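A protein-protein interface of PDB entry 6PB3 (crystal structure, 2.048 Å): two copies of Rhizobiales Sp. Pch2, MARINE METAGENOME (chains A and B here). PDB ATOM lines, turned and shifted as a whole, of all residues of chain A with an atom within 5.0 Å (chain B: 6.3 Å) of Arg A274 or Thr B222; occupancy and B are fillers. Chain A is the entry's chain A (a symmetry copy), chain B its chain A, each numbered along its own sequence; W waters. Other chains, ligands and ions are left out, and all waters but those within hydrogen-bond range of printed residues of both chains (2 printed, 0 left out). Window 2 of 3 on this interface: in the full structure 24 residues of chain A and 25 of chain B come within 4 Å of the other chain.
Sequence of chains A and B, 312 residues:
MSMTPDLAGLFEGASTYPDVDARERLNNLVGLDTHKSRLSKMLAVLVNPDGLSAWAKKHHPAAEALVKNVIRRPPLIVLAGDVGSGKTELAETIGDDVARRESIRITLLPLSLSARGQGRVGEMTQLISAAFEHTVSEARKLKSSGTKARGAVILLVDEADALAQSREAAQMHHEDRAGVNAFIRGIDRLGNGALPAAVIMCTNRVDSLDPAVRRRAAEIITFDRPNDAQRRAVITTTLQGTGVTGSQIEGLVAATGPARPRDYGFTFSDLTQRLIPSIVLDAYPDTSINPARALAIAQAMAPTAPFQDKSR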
ATOM      1  N   SER A 269      -9.937  -0.532  28.467  1.00  0.00           N
ATOM      2  CA  SER A 269     -11.326  -0.102  28.328  1.00  0.00           C
ATOM      3  C   SER A 269     -12.262  -1.271  28.049  1.00  0.00           C
ATOM      4  O   SER A 269     -13.343  -1.362  28.646  1.00  0.00           O
ATOM      5  CB  SER A 269     -11.434   0.923  27.206  1.00  0.00           C
ATOM      6  OG  SER A 269     -12.765   1.366  27.098  1.00  0.00           O
ATOM      7  N   ASP A 270     -11.902  -2.146  27.104  1.00  0.00           N
ATOM      8  CA  ASP A 270     -12.735  -3.322  26.840  1.00  0.00           C
ATOM      9  C   ASP A 270     -12.973  -4.142  28.108  1.00  0.00           C
ATOM     10  O   ASP A 270     -14.047  -4.728  28.279  1.00  0.00           O
ATOM     11  CB  ASP A 270     -12.100  -4.196  25.756  1.00  0.00           C
ATOM     12  CG  ASP A 270     -12.039  -3.498  24.387  1.00  0.00           C
ATOM     13  OD1 ASP A 270     -12.816  -2.533  24.155  1.00  0.00           O
ATOM     14  OD2 ASP A 270     -11.236  -3.939  23.526  1.00  0.00           O
ATOM     15  N   LEU A 271     -12.000  -4.184  29.023  1.00  0.00           N
ATOM     16  CA  LEU A 271     -12.243  -4.937  30.251  1.00  0.00           C
ATOM     17  C   LEU A 271     -13.145  -4.163  31.208  1.00  0.00           C
ATOM     18  O   LEU A 271     -14.093  -4.723  31.764  1.00  0.00           O
ATOM     19  CB  LEU A 271     -10.917  -5.299  30.934  1.00  0.00           C
ATOM     20  CG  LEU A 271     -10.008  -6.282  30.184  1.00  0.00           C
ATOM     21  CD1 LEU A 271      -8.630  -6.360  30.831  1.00  0.00           C
ATOM     22  CD2 LEU A 271     -10.661  -7.668  30.117  1.00  0.00           C
ATOM     23  N   THR A 272     -12.855  -2.882  31.432  1.00  0.00           N
ATOM     24  CA  THR A 272     -13.487  -2.161  32.534  1.00  0.00           C
ATOM     25  C   THR A 272     -14.816  -1.543  32.140  1.00  0.00           C
ATOM     26  O   THR A 272     -15.720  -1.470  32.976  1.00  0.00           O
ATOM     27  CB  THR A 272     -12.556  -1.064  33.078  1.00  0.00           C
ATOM     28  OG1 THR A 272     -12.218  -0.130  32.036  1.00  0.00           O
ATOM     29  CG2 THR A 272     -11.252  -1.659  33.646  1.00  0.00           C
ATOM     30  N   GLN A 273     -14.963  -1.102  30.889  1.00  0.00           N
ATOM     31  CA  GLN A 273     -16.185  -0.431  30.450  1.00  0.00           C
ATOM     32  C   GLN A 273     -17.129  -1.321  29.646  1.00  0.00           C
ATOM     33  O   GLN A 273     -18.269  -0.903  29.376  1.00  0.00           O
ATOM     34  CB  GLN A 273     -15.826   0.815  29.624  1.00  0.00           C
ATOM     35  CG  GLN A 273     -15.024   1.888  30.431  1.00  0.00           C
ATOM     36  CD  GLN A 273     -14.666   3.080  29.563  1.00  0.00           C
ATOM     37  OE1 GLN A 273     -13.701   3.033  28.805  1.00  0.00           O
ATOM     38  NE2 GLN A 273     -15.462   4.132  29.634  1.00  0.00           N
ATOM     39  N   ARG A 274     -16.700  -2.519  29.239  1.00  0.00           N
ATOM     40  CA  ARG A 274     -17.603  -3.427  28.530  1.00  0.00           C
ATOM     41  C   ARG A 274     -17.737  -4.765  29.239  1.00  0.00           C
ATOM     42  O   ARG A 274     -18.837  -5.107  29.681  1.00  0.00           O
ATOM     43  CB  ARG A 274     -17.144  -3.634  27.075  1.00  0.00           C
ATOM     44  CG  ARG A 274     -17.022  -2.335  26.261  1.00  0.00           C
ATOM     45  CD  ARG A 274     -16.308  -2.542  24.919  1.00  0.00           C
ATOM     46  NE  ARG A 274     -17.034  -3.444  24.020  1.00  0.00           N
ATOM     47  CZ  ARG A 274     -16.454  -4.178  23.072  1.00  0.00           C
ATOM     48  NH1 ARG A 274     -15.131  -4.126  22.903  1.00  0.00           N
ATOM     49  NH2 ARG A 274     -17.190  -4.968  22.294  1.00  0.00           N
ATOM     50  N   LEU A 275     -16.642  -5.517  29.394  1.00  0.00           N
ATOM     51  CA  LEU A 275     -16.779  -6.898  29.832  1.00  0.00           C
ATOM     52  C   LEU A 275     -17.209  -6.972  31.290  1.00  0.00           C
ATOM     53  O   LEU A 275     -18.122  -7.724  31.638  1.00  0.00           O
ATOM     54  CB  LEU A 275     -15.476  -7.663  29.624  1.00  0.00           C
ATOM     55  CG  LEU A 275     -15.456  -9.075  30.208  1.00  0.00           C
ATOM     56  CD1 LEU A 275     -16.487 -10.010  29.570  1.00  0.00           C
ATOM     57  CD2 LEU A 275     -14.057  -9.655  30.091  1.00  0.00           C
ATOM     58  N   ILE A 276     -16.559  -6.204  32.166  1.00  0.00           N
ATOM     59  CA  ILE A 276     -16.904  -6.263  33.592  1.00  0.00           C
ATOM     60  C   ILE A 276     -18.365  -5.881  33.835  1.00  0.00           C
ATOM     61  O   ILE A 276     -19.091  -6.671  34.456  1.00  0.00           O
ATOM     62  CB  ILE A 276     -15.916  -5.436  34.422  1.00  0.00           C
ATOM     63  CG1 ILE A 276     -14.587  -6.193  34.601  1.00  0.00           C
ATOM     64  CG2 ILE A 276     -16.524  -5.111  35.801  1.00  0.00           C
ATOM     65  CD1 ILE A 276     -13.464  -5.308  35.112  1.00  0.00           C
ATOM     66  N   PRO A 277     -18.868  -4.740  33.352  1.00  0.00           N
ATOM     67  CA  PRO A 277     -20.299  -4.471  33.525  1.00  0.00           C
ATOM     68  C   PRO A 277     -21.181  -5.582  32.991  1.00  0.00           C
ATOM     69  O   PRO A 277     -22.151  -5.956  33.663  1.00  0.00           O
ATOM     70  CB  PRO A 277     -20.501  -3.159  32.744  1.00  0.00           C
ATOM     71  CG  PRO A 277     -19.227  -2.488  32.727  1.00  0.00           C
ATOM     72  CD  PRO A 277     -18.191  -3.616  32.676  1.00  0.00           C
ATOM     73  N   SER A 278     -20.870  -6.120  31.800  1.00  0.00           N
ATOM     74  CA  SER A 278     -21.722  -7.143  31.200  1.00  0.00           C
ATOM     75  C   SER A 278     -21.793  -8.374  32.086  1.00  0.00           C
ATOM     76  O   SER A 278     -22.839  -9.017  32.188  1.00  0.00           O
ATOM     77  CB  SER A 278     -21.205  -7.533  29.808  1.00  0.00           C
ATOM     78  OG  SER A 278     -21.203  -6.423  28.916  1.00  0.00           O
ATOM     79  N   MET A 301     -17.767 -11.243  22.658  1.00  0.00           N
ATOM     80  CA  MET A 301     -17.463  -9.836  22.612  1.00  0.00           C
ATOM     81  C   MET A 301     -16.172  -9.614  21.815  1.00  0.00           C
ATOM     82  O   MET A 301     -15.147 -10.243  22.090  1.00  0.00           O
ATOM     83  CB  MET A 301     -17.353  -9.301  24.043  1.00  0.00           C
ATOM     84  CG  MET A 301     -17.002  -7.840  24.157  1.00  0.00           C
ATOM     85  SD  MET A 301     -16.836  -7.373  26.058  1.00  0.00           S
ATOM     86  CE  MET A 301     -18.766  -7.477  26.520  1.00  0.00           C
ATOM     87  N   ALA A 302     -16.227  -8.716  20.823  1.00  0.00           N
ATOM     88  CA  ALA A 302     -15.027  -8.476  20.022  1.00  0.00           C
ATOM     89  C   ALA A 302     -14.248  -7.286  20.566  1.00  0.00           C
ATOM     90  O   ALA A 302     -14.848  -6.288  20.974  1.00  0.00           O
ATOM     91  CB  ALA A 302     -15.370  -8.218  18.548  1.00  0.00           C
ATOM     92  N   PRO A 303     -12.917  -7.363  20.564  1.00  0.00           N
ATOM     93  CA  PRO A 303     -12.101  -6.266  21.101  1.00  0.00           C
ATOM     94  C   PRO A 303     -12.237  -5.007  20.261  1.00  0.00           C
ATOM     95  O   PRO A 303     -12.636  -5.044  19.096  1.00  0.00           O
ATOM     96  CB  PRO A 303     -10.666  -6.810  21.035  1.00  0.00           C
ATOM     97  CG  PRO A 303     -10.804  -8.283  20.845  1.00  0.00           C
ATOM     98  CD  PRO A 303     -12.096  -8.499  20.113  1.00  0.00           C
ATOM     99  N   THR A 304     -11.900  -3.873  20.876  1.00  0.00           N
ATOM    100  CA  THR A 304     -11.833  -2.630  20.126  1.00  0.00           C
ATOM    101  C   THR A 304     -10.715  -2.722  19.091  1.00  0.00           C
ATOM    102  O   THR A 304      -9.579  -3.082  19.413  1.00  0.00           O
ATOM    103  CB  THR A 304     -11.600  -1.448  21.067  1.00  0.00           C
ATOM    104  OG1 THR A 304     -12.671  -1.368  22.019  1.00  0.00           O
ATOM    105  CG2 THR A 304     -11.562  -0.144  20.275  1.00  0.00           C
ATOM    106  N   HIS B  35     -28.344  -6.499  24.212  1.00  0.00           N
ATOM    107  CA  HIS B  35     -28.138  -5.054  24.304  1.00  0.00           C
ATOM    108  C   HIS B  35     -29.225  -4.387  25.144  1.00  0.00           C
ATOM    109  O   HIS B  35     -28.942  -3.443  25.897  1.00  0.00           O
ATOM    110  CB  HIS B  35     -28.081  -4.432  22.904  1.00  0.00           C
ATOM    111  CG  HIS B  35     -27.135  -5.123  21.970  1.00  0.00           C
ATOM    112  ND1 HIS B  35     -27.382  -6.378  21.461  1.00  0.00           N
ATOM    113  CD2 HIS B  35     -25.930  -4.746  21.472  1.00  0.00           C
ATOM    114  CE1 HIS B  35     -26.383  -6.738  20.673  1.00  0.00           C
ATOM    115  NE2 HIS B  35     -25.489  -5.765  20.663  1.00  0.00           N
ATOM    116  N   ARG B  38     -28.537  -5.246  28.976  1.00  0.00           N
ATOM    117  CA  ARG B  38     -27.420  -4.485  29.532  1.00  0.00           C
ATOM    118  C   ARG B  38     -27.764  -3.004  29.643  1.00  0.00           C
ATOM    119  O   ARG B  38     -27.525  -2.376  30.680  1.00  0.00           O
ATOM    120  CB  ARG B  38     -26.164  -4.674  28.684  1.00  0.00           C
ATOM    121  CG  ARG B  38     -25.631  -6.078  28.679  1.00  0.00           C
ATOM    122  CD  ARG B  38     -24.387  -6.176  27.775  1.00  0.00           C
ATOM    123  NE  ARG B  38     -24.007  -7.570  27.588  1.00  0.00           N
ATOM    124  CZ  ARG B  38     -23.095  -7.996  26.720  1.00  0.00           C
ATOM    125  NH1 ARG B  38     -22.449  -7.141  25.942  1.00  0.00           N
ATOM    126  NH2 ARG B  38     -22.828  -9.288  26.636  1.00  0.00           N
ATOM    127  N   VAL B  78     -22.678   4.680  26.575  1.00  0.00           N
ATOM    128  CA  VAL B  78     -22.387   4.911  25.166  1.00  0.00           C
ATOM    129  C   VAL B  78     -22.895   3.717  24.370  1.00  0.00           C
ATOM    130  O   VAL B  78     -22.574   2.568  24.695  1.00  0.00           O
ATOM    131  CB  VAL B  78     -20.882   5.133  24.945  1.00  0.00           C
ATOM    132  CG1 VAL B  78     -20.543   5.149  23.444  1.00  0.00           C
ATOM    133  CG2 VAL B  78     -20.462   6.457  25.560  1.00  0.00           C
ATOM    134  N   LEU B  79     -23.693   3.987  23.340  1.00  0.00           N
ATOM    135  CA  LEU B  79     -24.095   2.988  22.354  1.00  0.00           C
ATOM    136  C   LEU B  79     -23.312   3.262  21.087  1.00  0.00           C
ATOM    137  O   LEU B  79     -23.483   4.321  20.475  1.00  0.00           O
ATOM    138  CB  LEU B  79     -25.604   3.039  22.076  1.00  0.00           C
ATOM    139  CG  LEU B  79     -26.588   2.997  23.241  1.00  0.00           C
ATOM    140  CD1 LEU B  79     -28.030   2.803  22.698  1.00  0.00           C
ATOM    141  CD2 LEU B  79     -26.237   1.900  24.219  1.00  0.00           C
ATOM    142  N   ALA B  80     -22.460   2.313  20.692  1.00  0.00           N
ATOM    143  CA  ALA B  80     -21.539   2.509  19.577  1.00  0.00           C
ATOM    144  C   ALA B  80     -21.665   1.365  18.580  1.00  0.00           C
ATOM    145  O   ALA B  80     -21.806   0.205  18.980  1.00  0.00           O
ATOM    146  CB  ALA B  80     -20.086   2.581  20.072  1.00  0.00           C
ATOM    147  N   GLY B  81     -21.602   1.674  17.292  1.00  0.00           N
ATOM    148  CA  GLY B  81     -21.548   0.636  16.285  1.00  0.00           C
ATOM    149  C   GLY B  81     -22.274   1.018  15.007  1.00  0.00           C
ATOM    150  O   GLY B  81     -22.615   2.176  14.779  1.00  0.00           O
ATOM    151  N   ALA B 218     -19.825   4.830  31.934  1.00  0.00           N
ATOM    152  CA  ALA B 218     -19.959   3.725  32.868  1.00  0.00           C
ATOM    153  C   ALA B 218     -20.004   2.415  32.117  1.00  0.00           C
ATOM    154  O   ALA B 218     -19.445   1.413  32.567  1.00  0.00           O
ATOM    155  CB  ALA B 218     -21.218   3.890  33.708  1.00  0.00           C
ATOM    156  N   GLU B 219     -20.652   2.410  30.961  1.00  0.00           N
ATOM    157  CA  GLU B 219     -20.640   1.230  30.120  1.00  0.00           C
ATOM    158  C   GLU B 219     -20.678   1.662  28.671  1.00  0.00           C
ATOM    159  O   GLU B 219     -21.344   2.638  28.319  1.00  0.00           O
ATOM    160  CB  GLU B 219     -21.829   0.292  30.419  1.00  0.00           C
ATOM    161  CG  GLU B 219     -21.722  -1.035  29.681  1.00  0.00           C
ATOM    162  CD  GLU B 219     -22.876  -1.970  29.940  1.00  0.00           C
ATOM    163  OE1 GLU B 219     -23.833  -1.583  30.627  1.00  0.00           O
ATOM    164  OE2 GLU B 219     -22.829  -3.108  29.439  1.00  0.00           O
ATOM    165  N   ILE B 220     -19.949   0.924  27.843  1.00  0.00           N
ATOM    166  CA  ILE B 220     -20.017   1.024  26.395  1.00  0.00           C
ATOM    167  C   ILE B 220     -20.651  -0.262  25.889  1.00  0.00           C
ATOM    168  O   ILE B 220     -20.190  -1.359  26.228  1.00  0.00           O
ATOM    169  CB  ILE B 220     -18.621   1.230  25.785  1.00  0.00           C
ATOM    170  CG1 ILE B 220     -17.933   2.473  26.398  1.00  0.00           C
ATOM    171  CG2 ILE B 220     -18.729   1.306  24.255  1.00  0.00           C
ATOM    172  CD1 ILE B 220     -16.453   2.674  25.935  1.00  0.00           C
ATOM    173  N   ILE B 221     -21.698  -0.135  25.080  1.00  0.00           N
ATOM    174  CA  ILE B 221     -22.441  -1.277  24.548  1.00  0.00           C
ATOM    175  C   ILE B 221     -22.293  -1.237  23.044  1.00  0.00           C
ATOM    176  O   ILE B 221     -22.655  -0.237  22.405  1.00  0.00           O
ATOM    177  CB  ILE B 221     -23.923  -1.243  24.950  1.00  0.00           C
ATOM    178  CG1 ILE B 221     -24.081  -1.332  26.470  1.00  0.00           C
ATOM    179  CG2 ILE B 221     -24.735  -2.392  24.249  1.00  0.00           C
ATOM    180  CD1 ILE B 221     -25.544  -1.056  26.908  1.00  0.00           C
ATOM    181  N   THR B 222     -21.779  -2.317  22.469  1.00  0.00           N
ATOM    182  CA  THR B 222     -21.382  -2.280  21.076  1.00  0.00           C
ATOM    183  C   THR B 222     -22.379  -3.026  20.199  1.00  0.00           C
ATOM    184  O   THR B 222     -22.902  -4.079  20.583  1.00  0.00           O
ATOM    185  CB  THR B 222     -19.968  -2.841  20.896  1.00  0.00           C
ATOM    186  OG1 THR B 222     -19.888  -4.164  21.447  1.00  0.00           O
ATOM    187  CG2 THR B 222     -18.957  -1.931  21.629  1.00  0.00           C
ATOM    188  N   PHE B 223     -22.624  -2.458  19.017  1.00  0.00           N
ATOM    189  CA  PHE B 223     -23.527  -2.968  17.995  1.00  0.00           C
ATOM    190  C   PHE B 223     -22.661  -3.237  16.770  1.00  0.00           C
ATOM    191  O   PHE B 223     -22.453  -2.371  15.915  1.00  0.00           O
ATOM    192  CB  PHE B 223     -24.652  -1.973  17.685  1.00  0.00           C
ATOM    193  CG  PHE B 223     -25.507  -1.636  18.876  1.00  0.00           C
ATOM    194  CD1 PHE B 223     -24.993  -0.895  19.924  1.00  0.00           C
ATOM    195  CD2 PHE B 223     -26.822  -2.073  18.953  1.00  0.00           C
ATOM    196  CE1 PHE B 223     -25.770  -0.602  21.038  1.00  0.00           C
ATOM    197  CE2 PHE B 223     -27.609  -1.775  20.062  1.00  0.00           C
ATOM    198  CZ  PHE B 223     -27.089  -1.033  21.096  1.00  0.00           C
ATOM    199  N   ASP B 224     -22.136  -4.435  16.692  1.00  0.00           N
ATOM    200  CA  ASP B 224     -21.431  -4.851  15.503  1.00  0.00           C
ATOM    201  C   ASP B 224     -22.234  -5.961  14.852  1.00  0.00           C
ATOM    202  O   ASP B 224     -23.407  -6.186  15.189  1.00  0.00           O
ATOM    203  CB  ASP B 224     -19.994  -5.266  15.826  1.00  0.00           C
ATOM    204  CG  ASP B 224     -19.870  -5.956  17.163  1.00  0.00           C
ATOM    205  OD1 ASP B 224     -20.628  -6.914  17.402  1.00  0.00           O
ATOM    206  OD2 ASP B 224     -19.000  -5.545  17.967  1.00  0.00           O
HETATM  207  O   HOH W   1     -24.748  -8.800  30.365  1.00  0.00           O
HETATM  208  O   HOH W   2     -20.276  -4.459  24.234  1.00  0.00           O
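Among the printed residues, pairs that only touch across the chains: Gln A273 with Glu B219 (3.3 Å), Arg A274 with Ile B220 (3.3 Å), Ser A278 with Glu B219 (3.7 Å), Met A301 with Arg B38 (3.7 Å), Pro A277 with Glu B219 (3.9 Å) and Pro A277 with Ala B218 (3.9 Å).
The backbone NH (N) of Ile B220 is in hydrogen-bond range of the backbone carbonyl oxygen (O) of Gln A273, 2.9 Å away.
The side-chain hydroxyl of Thr B222 sits at hydrogen-bond distance from the guanidinium group of Arg A274 (2.9 Å).
OG of Ser A278 lies close to NH1 of Arg B38, 3.3 Å away.
Of the 14 printed residues of chain A, 5 touch a printed residue of chain B.
Hydrophobic or aromatic side chains of chain A that line the printed part of chain B: Pro A277 and Met A301.
Hydrophobic or aromatic side chains of chain B within 4 Å of the printed part of chain A: Ile B220.
Among the printed residues, 9 pairs touch across the chains.
Among the printed residues, no Asp or Glu carboxylate lies within 4 Å of a Lys or Arg side-chain nitrogen of the other chain.
Of chain B, only Ile B220 (3.3 Å) and Thr B222 (2.9 Å) come within 4 Å of Arg A274.
Thr B222 touches one residue of chain A.
Printed residues of chain B within 4 Å of Met A301: Arg B38 (3.7 Å).
Of the printed residues of chain A, Glu B219 touches Gln A273 (3.3 Å), Pro A277 (3.9 Å) and Ser A278 (3.7 Å).
Printed residues of chain A within 4 Å of Ile B220: Gln A273 and Arg A274.
Of the printed residues of chain B, Ser A278 touches Arg B38 and Glu B219.
Gly B81 touches none of the printed residues of chain A.
The nearest residue of chain B that does not touch Arg A274 is Glu B219 (4.5 Å).
The nearest printed residue of chain A that does not touch Arg B38 is Arg A274 (5.6 Å).
Water W1 bridges the backbone carbonyl oxygen (O) of Ser A278 (2.6 Å) and the guanidinium group (NE) of Arg B38 (3.1 Å).
Water W2 lies within hydrogen-bond range of OG1 of Thr B222 (2.8 Å) and NE of Arg A274 (3.4 Å).
No position is printed for both chains.
Of the 9 pairs that touch across the chains among the printed residues, none has its exchanged pair printed and touching as well.
OG of Ser A278 sits at hydrogen-bond distance from O of Arg A274, at 2.8 Å.
O of Ala A302 lies within hydrogen-bond range of NH1 of Arg A274 (2.9 Å).
The backbone carbonyl oxygen (O) of Glu B219 is in hydrogen-bond range of the backbone NH (N) of Val B78, 3.0 Å away.
OD1 of Asp A270 lies within salt-bridge range of NH1 of Arg A274.
OE1 of Gln A273 is in hydrogen-bond range of OG of Ser A269, at 2.6 Å.
NE2 of His B35 lies within hydrogen-bond range of O of Thr B222.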
